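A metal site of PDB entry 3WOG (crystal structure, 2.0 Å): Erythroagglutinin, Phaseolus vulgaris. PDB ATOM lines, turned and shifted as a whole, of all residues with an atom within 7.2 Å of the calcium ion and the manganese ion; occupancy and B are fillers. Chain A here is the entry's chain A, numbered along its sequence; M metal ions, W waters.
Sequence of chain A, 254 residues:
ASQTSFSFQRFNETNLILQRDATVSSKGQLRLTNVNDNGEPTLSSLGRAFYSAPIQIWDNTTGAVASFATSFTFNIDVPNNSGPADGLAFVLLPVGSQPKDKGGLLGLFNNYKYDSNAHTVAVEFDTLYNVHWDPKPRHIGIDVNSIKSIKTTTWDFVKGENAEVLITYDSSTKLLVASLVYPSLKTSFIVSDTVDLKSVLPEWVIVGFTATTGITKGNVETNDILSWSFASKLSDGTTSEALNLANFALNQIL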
ATOM      1  N   ASP A  86     -28.578 -22.834  12.424  1.00  0.00           N
ATOM      2  CA  ASP A  86     -28.402 -23.317  11.038  1.00  0.00           C
ATOM      3  C   ASP A  86     -29.421 -22.742  10.051  1.00  0.00           C
ATOM      4  O   ASP A  86     -29.193 -22.695   8.846  1.00  0.00           O
ATOM      5  CB  ASP A  86     -28.504 -24.827  11.015  1.00  0.00           C
ATOM      6  CG  ASP A  86     -27.168 -25.483  11.162  1.00  0.00           C
ATOM      7  OD1 ASP A  86     -26.371 -25.420  10.192  1.00  0.00           O
ATOM      8  OD2 ASP A  86     -26.916 -26.043  12.261  1.00  0.00           O
ATOM      9  N   GLY A  87     -30.578 -22.354  10.578  1.00  0.00           N
ATOM     10  CA  GLY A  87     -31.571 -21.629   9.785  1.00  0.00           C
ATOM     11  C   GLY A  87     -32.963 -22.137  10.104  1.00  0.00           C
ATOM     12  O   GLY A  87     -33.163 -22.895  11.073  1.00  0.00           O
ATOM     13  N   GLY A 103     -29.033 -29.714  13.304  1.00  0.00           N
ATOM     14  CA  GLY A 103     -27.989 -28.975  12.586  1.00  0.00           C
ATOM     15  C   GLY A 103     -28.355 -28.638  11.159  1.00  0.00           C
ATOM     16  O   GLY A 103     -29.478 -28.211  10.877  1.00  0.00           O
ATOM     17  N   GLY A 104     -27.415 -28.831  10.236  1.00  0.00           N
ATOM     18  CA  GLY A 104     -27.628 -28.451   8.841  1.00  0.00           C
ATOM     19  C   GLY A 104     -28.694 -29.240   8.095  1.00  0.00           C
ATOM     20  O   GLY A 104     -29.062 -28.885   6.988  1.00  0.00           O
ATOM     21  N   LEU A 105     -29.177 -30.331   8.669  1.00  0.00           N
ATOM     22  CA  LEU A 105     -30.270 -31.092   8.058  1.00  0.00           C
ATOM     23  C   LEU A 105     -31.658 -30.542   8.430  1.00  0.00           C
ATOM     24  O   LEU A 105     -32.698 -31.041   7.964  1.00  0.00           O
ATOM     25  CB  LEU A 105     -30.117 -32.581   8.416  1.00  0.00           C
ATOM     26  CG  LEU A 105     -28.808 -33.186   7.880  1.00  0.00           C
ATOM     27  CD1 LEU A 105     -28.582 -34.631   8.355  1.00  0.00           C
ATOM     28  CD2 LEU A 105     -28.739 -33.116   6.371  1.00  0.00           C
ATOM     29  N   LEU A 106     -31.648 -29.497   9.259  1.00  0.00           N
ATOM     30  CA  LEU A 106     -32.842 -28.684   9.583  1.00  0.00           C
ATOM     31  C   LEU A 106     -34.036 -29.437  10.202  1.00  0.00           C
ATOM     32  O   LEU A 106     -35.157 -28.938  10.174  1.00  0.00           O
ATOM     33  CB  LEU A 106     -33.307 -27.877   8.366  1.00  0.00           C
ATOM     34  CG  LEU A 106     -32.283 -26.916   7.752  1.00  0.00           C
ATOM     35  CD1 LEU A 106     -32.826 -26.268   6.470  1.00  0.00           C
ATOM     36  CD2 LEU A 106     -31.866 -25.838   8.745  1.00  0.00           C
ATOM     37  N   GLU A 124     -36.248 -23.079   2.539  1.00  0.00           N
ATOM     38  CA  GLU A 124     -35.276 -22.885   3.604  1.00  0.00           C
ATOM     39  C   GLU A 124     -34.663 -21.496   3.592  1.00  0.00           C
ATOM     40  O   GLU A 124     -34.473 -20.882   2.534  1.00  0.00           O
ATOM     41  CB  GLU A 124     -34.132 -23.931   3.502  1.00  0.00           C
ATOM     42  CG  GLU A 124     -33.274 -23.885   2.243  1.00  0.00           C
ATOM     43  CD  GLU A 124     -32.020 -24.755   2.355  1.00  0.00           C
ATOM     44  OE1 GLU A 124     -32.162 -25.923   2.813  1.00  0.00           O
ATOM     45  OE2 GLU A 124     -30.884 -24.271   2.052  1.00  0.00           O
ATOM     46  N   PHE A 125     -34.315 -21.021   4.781  1.00  0.00           N
ATOM     47  CA  PHE A 125     -33.612 -19.777   4.952  1.00  0.00           C
ATOM     48  C   PHE A 125     -32.389 -20.234   5.727  1.00  0.00           C
ATOM     49  O   PHE A 125     -32.444 -20.448   6.931  1.00  0.00           O
ATOM     50  CB  PHE A 125     -34.527 -18.773   5.687  1.00  0.00           C
ATOM     51  CG  PHE A 125     -35.749 -18.424   4.887  1.00  0.00           C
ATOM     52  CD1 PHE A 125     -35.750 -17.355   3.986  1.00  0.00           C
ATOM     53  CD2 PHE A 125     -36.880 -19.237   4.949  1.00  0.00           C
ATOM     54  CE1 PHE A 125     -36.860 -17.079   3.199  1.00  0.00           C
ATOM     55  CE2 PHE A 125     -37.995 -18.957   4.170  1.00  0.00           C
ATOM     56  CZ  PHE A 125     -37.978 -17.890   3.293  1.00  0.00           C
ATOM     57  N   ASP A 126     -31.309 -20.454   4.971  1.00  0.00           N
ATOM     58  CA  ASP A 126     -30.139 -21.240   5.422  1.00  0.00           C
ATOM     59  C   ASP A 126     -29.029 -20.249   5.769  1.00  0.00           C
ATOM     60  O   ASP A 126     -28.560 -19.496   4.911  1.00  0.00           O
ATOM     61  CB  ASP A 126     -29.709 -22.209   4.264  1.00  0.00           C
ATOM     62  CG  ASP A 126     -28.630 -23.214   4.678  1.00  0.00           C
ATOM     63  OD1 ASP A 126     -27.986 -22.960   5.709  1.00  0.00           O
ATOM     64  OD2 ASP A 126     -28.424 -24.258   3.938  1.00  0.00           O
ATOM     65  N   THR A 127     -28.634 -20.206   7.043  1.00  0.00           N
ATOM     66  CA  THR A 127     -27.655 -19.209   7.482  1.00  0.00           C
ATOM     67  C   THR A 127     -26.250 -19.786   7.658  1.00  0.00           C
ATOM     68  O   THR A 127     -25.347 -19.102   8.134  1.00  0.00           O
ATOM     69  CB  THR A 127     -28.056 -18.596   8.837  1.00  0.00           C
ATOM     70  OG1 THR A 127     -28.090 -19.633   9.814  1.00  0.00           O
ATOM     71  CG2 THR A 127     -29.439 -17.879   8.757  1.00  0.00           C
ATOM     72  N   LEU A 128     -26.053 -21.053   7.312  1.00  0.00           N
ATOM     73  CA  LEU A 128     -24.729 -21.646   7.479  1.00  0.00           C
ATOM     74  C   LEU A 128     -24.363 -22.551   6.312  1.00  0.00           C
ATOM     75  O   LEU A 128     -25.086 -23.505   5.988  1.00  0.00           O
ATOM     76  CB  LEU A 128     -24.656 -22.410   8.803  1.00  0.00           C
ATOM     77  CG  LEU A 128     -23.253 -23.012   9.032  1.00  0.00           C
ATOM     78  CD1 LEU A 128     -22.659 -22.550  10.350  1.00  0.00           C
ATOM     79  CD2 LEU A 128     -23.182 -24.524   8.835  1.00  0.00           C
ATOM     80  N   TYR A 129     -23.230 -22.216   5.686  1.00  0.00           N
ATOM     81  CA  TYR A 129     -22.649 -22.998   4.603  1.00  0.00           C
ATOM     82  C   TYR A 129     -22.233 -24.409   5.033  1.00  0.00           C
ATOM     83  O   TYR A 129     -21.351 -24.596   5.874  1.00  0.00           O
ATOM     84  CB  TYR A 129     -21.446 -22.239   4.024  1.00  0.00           C
ATOM     85  CG  TYR A 129     -20.520 -23.009   3.082  1.00  0.00           C
ATOM     86  CD1 TYR A 129     -20.977 -23.470   1.851  1.00  0.00           C
ATOM     87  CD2 TYR A 129     -19.178 -23.209   3.415  1.00  0.00           C
ATOM     88  CE1 TYR A 129     -20.124 -24.143   0.967  1.00  0.00           C
ATOM     89  CE2 TYR A 129     -18.312 -23.879   2.562  1.00  0.00           C
ATOM     90  CZ  TYR A 129     -18.782 -24.341   1.337  1.00  0.00           C
ATOM     91  OH  TYR A 129     -17.929 -24.987   0.489  1.00  0.00           O
ATOM     92  N   ASN A 130     -22.876 -25.406   4.445  1.00  0.00           N
ATOM     93  CA  ASN A 130     -22.533 -26.787   4.703  1.00  0.00           C
ATOM     94  C   ASN A 130     -21.796 -27.294   3.482  1.00  0.00           C
ATOM     95  O   ASN A 130     -22.399 -27.437   2.395  1.00  0.00           O
ATOM     96  CB  ASN A 130     -23.793 -27.612   4.970  1.00  0.00           C
ATOM     97  CG  ASN A 130     -24.404 -27.318   6.320  1.00  0.00           C
ATOM     98  OD1 ASN A 130     -25.409 -26.587   6.424  1.00  0.00           O
ATOM     99  ND2 ASN A 130     -23.799 -27.856   7.380  1.00  0.00           N
ATOM    100  N   VAL A 131     -20.487 -27.524   3.647  1.00  0.00           N
ATOM    101  CA  VAL A 131     -19.582 -27.789   2.517  1.00  0.00           C
ATOM    102  C   VAL A 131     -20.042 -28.883   1.536  1.00  0.00           C
ATOM    103  O   VAL A 131     -19.794 -28.800   0.321  1.00  0.00           O
ATOM    104  CB  VAL A 131     -18.142 -28.106   3.034  1.00  0.00           C
ATOM    105  CG1 VAL A 131     -18.118 -29.379   3.874  1.00  0.00           C
ATOM    106  CG2 VAL A 131     -17.165 -28.201   1.883  1.00  0.00           C
ATOM    107  N   TRP A 133     -22.989 -29.681   0.504  1.00  0.00           N
ATOM    108  CA  TRP A 133     -24.148 -29.439  -0.380  1.00  0.00           C
ATOM    109  C   TRP A 133     -24.570 -28.021  -0.626  1.00  0.00           C
ATOM    110  O   TRP A 133     -25.264 -27.769  -1.607  1.00  0.00           O
ATOM    111  CB  TRP A 133     -25.357 -30.238   0.078  1.00  0.00           C
ATOM    112  CG  TRP A 133     -25.874 -29.781   1.422  1.00  0.00           C
ATOM    113  CD1 TRP A 133     -26.682 -28.676   1.698  1.00  0.00           C
ATOM    114  CD2 TRP A 133     -25.611 -30.399   2.715  1.00  0.00           C
ATOM    115  NE1 TRP A 133     -26.936 -28.583   3.051  1.00  0.00           N
ATOM    116  CE2 TRP A 133     -26.324 -29.585   3.720  1.00  0.00           C
ATOM    117  CE3 TRP A 133     -24.894 -31.516   3.150  1.00  0.00           C
ATOM    118  CZ2 TRP A 133     -26.291 -29.897   5.068  1.00  0.00           C
ATOM    119  CZ3 TRP A 133     -24.882 -31.819   4.519  1.00  0.00           C
ATOM    120  CH2 TRP A 133     -25.570 -31.034   5.440  1.00  0.00           C
ATOM    121  N   ASP A 134     -24.217 -27.080   0.259  1.00  0.00           N
ATOM    122  CA  ASP A 134     -24.724 -25.696   0.139  1.00  0.00           C
ATOM    123  C   ASP A 134     -23.933 -24.836  -0.836  1.00  0.00           C
ATOM    124  O   ASP A 134     -22.718 -25.044  -1.002  1.00  0.00           O
ATOM    125  CB  ASP A 134     -24.678 -24.994   1.494  1.00  0.00           C
ATOM    126  CG  ASP A 134     -25.915 -25.270   2.362  1.00  0.00           C
ATOM    127  OD1 ASP A 134     -27.089 -25.399   1.864  1.00  0.00           O
ATOM    128  OD2 ASP A 134     -25.679 -25.320   3.590  1.00  0.00           O
ATOM    129  N   PRO A 135     -24.594 -23.828  -1.459  1.00  0.00           N
ATOM    130  CA  PRO A 135     -23.796 -22.736  -2.016  1.00  0.00           C
ATOM    131  C   PRO A 135     -23.146 -21.941  -0.874  1.00  0.00           C
ATOM    132  O   PRO A 135     -23.669 -21.917   0.246  1.00  0.00           O
ATOM    133  CB  PRO A 135     -24.824 -21.866  -2.771  1.00  0.00           C
ATOM    134  CG  PRO A 135     -26.166 -22.236  -2.199  1.00  0.00           C
ATOM    135  CD  PRO A 135     -26.054 -23.622  -1.616  1.00  0.00           C
ATOM    136  N   PRO A 137     -22.569 -18.537  -0.260  1.00  0.00           N
ATOM    137  CA  PRO A 137     -23.308 -17.441   0.376  1.00  0.00           C
ATOM    138  C   PRO A 137     -24.554 -17.983   1.112  1.00  0.00           C
ATOM    139  O   PRO A 137     -25.110 -19.006   0.715  1.00  0.00           O
ATOM    140  CB  PRO A 137     -23.751 -16.580  -0.809  1.00  0.00           C
ATOM    141  CG  PRO A 137     -22.891 -17.015  -1.980  1.00  0.00           C
ATOM    142  CD  PRO A 137     -22.646 -18.469  -1.733  1.00  0.00           C
ATOM    143  N   HIS A 139     -28.470 -18.140   1.851  1.00  0.00           N
ATOM    144  CA  HIS A 139     -29.340 -18.380   0.701  1.00  0.00           C
ATOM    145  C   HIS A 139     -30.765 -18.704   1.074  1.00  0.00           C
ATOM    146  O   HIS A 139     -31.020 -19.219   2.154  1.00  0.00           O
ATOM    147  CB  HIS A 139     -28.748 -19.502  -0.191  1.00  0.00           C
ATOM    148  CG  HIS A 139     -28.479 -20.823   0.541  1.00  0.00           C
ATOM    149  ND1 HIS A 139     -27.346 -21.060   1.216  1.00  0.00           N
ATOM    150  CD2 HIS A 139     -29.245 -22.003   0.618  1.00  0.00           C
ATOM    151  CE1 HIS A 139     -27.370 -22.298   1.741  1.00  0.00           C
ATOM    152  NE2 HIS A 139     -28.540 -22.890   1.373  1.00  0.00           N
ATOM    153  N   ILE A 140     -31.700 -18.360   0.190  1.00  0.00           N
ATOM    154  CA  ILE A 140     -33.056 -18.919   0.251  1.00  0.00           C
ATOM    155  C   ILE A 140     -33.024 -20.098  -0.708  1.00  0.00           C
ATOM    156  O   ILE A 140     -32.497 -19.969  -1.812  1.00  0.00           O
ATOM    157  CB  ILE A 140     -34.138 -17.896  -0.188  1.00  0.00           C
ATOM    158  CG1 ILE A 140     -34.002 -16.592   0.599  1.00  0.00           C
ATOM    159  CG2 ILE A 140     -35.536 -18.494  -0.025  1.00  0.00           C
ATOM    160  CD1 ILE A 140     -34.849 -15.452   0.054  1.00  0.00           C
ATOM    161  N   GLY A 141     -33.513 -21.253  -0.253  1.00  0.00           N
ATOM    162  CA  GLY A 141     -33.556 -22.458  -1.097  1.00  0.00           C
ATOM    163  C   GLY A 141     -34.922 -23.163  -1.162  1.00  0.00           C
ATOM    164  O   GLY A 141     -35.664 -23.184  -0.173  1.00  0.00           O
ATOM    165  N   ASP A 143     -36.450 -26.778  -1.415  1.00  0.00           N
ATOM    166  CA  ASP A 143     -36.024 -28.136  -1.125  1.00  0.00           C
ATOM    167  C   ASP A 143     -37.140 -29.103  -1.488  1.00  0.00           C
ATOM    168  O   ASP A 143     -38.290 -28.914  -1.060  1.00  0.00           O
ATOM    169  CB  ASP A 143     -35.702 -28.346   0.371  1.00  0.00           C
ATOM    170  CG  ASP A 143     -34.556 -27.465   0.865  1.00  0.00           C
ATOM    171  OD1 ASP A 143     -33.890 -26.809   0.042  1.00  0.00           O
ATOM    172  OD2 ASP A 143     -34.308 -27.453   2.103  1.00  0.00           O
ATOM    173  N   ILE A 147     -31.904 -32.046   1.343  1.00  0.00           N
ATOM    174  CA  ILE A 147     -31.286 -30.841   1.912  1.00  0.00           C
ATOM    175  C   ILE A 147     -30.519 -30.065   0.832  1.00  0.00           C
ATOM    176  O   ILE A 147     -30.197 -28.875   0.993  1.00  0.00           O
ATOM    177  CB  ILE A 147     -30.380 -31.191   3.129  1.00  0.00           C
ATOM    178  CG1 ILE A 147     -30.168 -29.985   4.064  1.00  0.00           C
ATOM    179  CG2 ILE A 147     -29.037 -31.766   2.671  1.00  0.00           C
ATOM    180  CD1 ILE A 147     -31.447 -29.326   4.559  1.00  0.00           C
ATOM    181  N   LYS A 148     -30.252 -30.738  -0.293  1.00  0.00           N
ATOM    182  CA  LYS A 148     -29.589 -30.086  -1.397  1.00  0.00           C
ATOM    183  C   LYS A 148     -30.643 -29.413  -2.255  1.00  0.00           C
ATOM    184  O   LYS A 148     -31.314 -30.078  -3.038  1.00  0.00           O
ATOM    185  CB  LYS A 148     -28.750 -31.063  -2.240  1.00  0.00           C
ATOM    186  CG  LYS A 148     -27.901 -30.341  -3.269  1.00  0.00           C
ATOM    187  CD  LYS A 148     -27.309 -31.249  -4.337  1.00  0.00           C
ATOM    188  CE  LYS A 148     -27.069 -30.413  -5.598  1.00  0.00           C
ATOM    189  NZ  LYS A 148     -26.300 -31.088  -6.679  1.00  0.00           N
ATOM    190  N   SER A 149     -30.780 -28.089  -2.114  1.00  0.00           N
ATOM    191  CA  SER A 149     -31.865 -27.347  -2.762  1.00  0.00           C
ATOM    192  C   SER A 149     -31.865 -27.514  -4.273  1.00  0.00           C
ATOM    193  O   SER A 149     -30.798 -27.535  -4.908  1.00  0.00           O
ATOM    194  CB  SER A 149     -31.807 -25.859  -2.405  1.00  0.00           C
ATOM    195  OG  SER A 149     -31.667 -25.689  -0.998  1.00  0.00           O
ATOM    196  N   THR A 152     -31.600 -22.122  -5.529  1.00  0.00           N
ATOM    197  CA  THR A 152     -31.236 -21.191  -4.454  1.00  0.00           C
ATOM    198  C   THR A 152     -31.059 -19.766  -4.992  1.00  0.00           C
ATOM    199  O   THR A 152     -30.888 -19.556  -6.195  1.00  0.00           O
ATOM    200  CB  THR A 152     -29.926 -21.586  -3.733  1.00  0.00           C
ATOM    201  OG1 THR A 152     -28.853 -21.592  -4.679  1.00  0.00           O
ATOM    202  CG2 THR A 152     -30.032 -22.973  -3.102  1.00  0.00           C
HETATM  203 CA    CA M   1     -26.856 -24.998   5.562  1.00  0.00          CA
HETATM  204 MN    MN M   2     -28.942 -24.694   2.072  1.00  0.00          MN
HETATM  205  O   HOH W   1     -29.288 -25.247   0.240  1.00  0.00           O
HETATM  206  O   HOH W   2     -27.453 -24.846   7.805  1.00  0.00           O
HETATM  207  O   HOH W   3     -28.267 -26.823   5.152  1.00  0.00           O
HETATM  208  O   HOH W   4     -29.524 -26.471   2.582  1.00  0.00           O
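A ring nitrogen (ND1) of His 139 is in hydrogen-bond range of the backbone carbonyl oxygen (O) of Pro 137 (3.1 Å). The side-chain carboxylate of Glu 124 lies close to the side-chain hydroxyl of Ser 149, at 3.5 Å. The side-chain carboxylate of Glu 124 sits close to the side-chain carboxylate of Asp 143, at 2.7 Å. N of Glu 124 sits at hydrogen-bond distance from O of Gly 141, 2.8 Å away. The side-chain carboxylate (OD1) of Asp 134 lies close to the indole nitrogen (NE1) of Trp 133 (3.4 Å).
Four residues have an atom within 4 Å of the calcium ion: Asp 126, Leu 128, Asn 130 and Asp 134. The nearest printed residue that does not touch the calcium ion is Trp 133 (4.4 Å).
Of the 26 residues printed, 4 come within 4 Å of the manganese ion. The nearest printed residue that does not touch the manganese ion is Ser 149 (4.2 Å).
The calcium ion is bound by OD1 of Asn 130 (2.3 Å), OD2 of Asp 134 (2.3 Å), water W2 (2.3 Å), OD1 of Asp 126 (2.3 Å), water W3 (2.3 Å), O of Leu 128 (2.4 Å) and OD2 of Asp 126 (2.4 Å).
The manganese ion is bound by water W4 (1.9 Å). The manganese ion is bound by water W1 (1.9 Å). The manganese ion is bound by NE2 of His 139 (2.0 Å). OD2 of Asp 126 is bound to the manganese ion (2.0 Å). The manganese ion is bound by the side-chain carboxylate (OE2) of Glu 124 (2.0 Å). OD1 of Asp 134 is bound to the manganese ion (2.0 Å).
Water W3 bridges the backbone carbonyl oxygen (O) of Gly 104 and the indole nitrogen (NE1) of Trp 133. Water W4 lies within hydrogen-bond range of the side-chain carboxylate of Glu 124 (2.7 Å), the backbone carbonyl oxygen of Ile 147 (3.0 Å) and the indole nitrogen of Trp 133 (3.4 Å).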
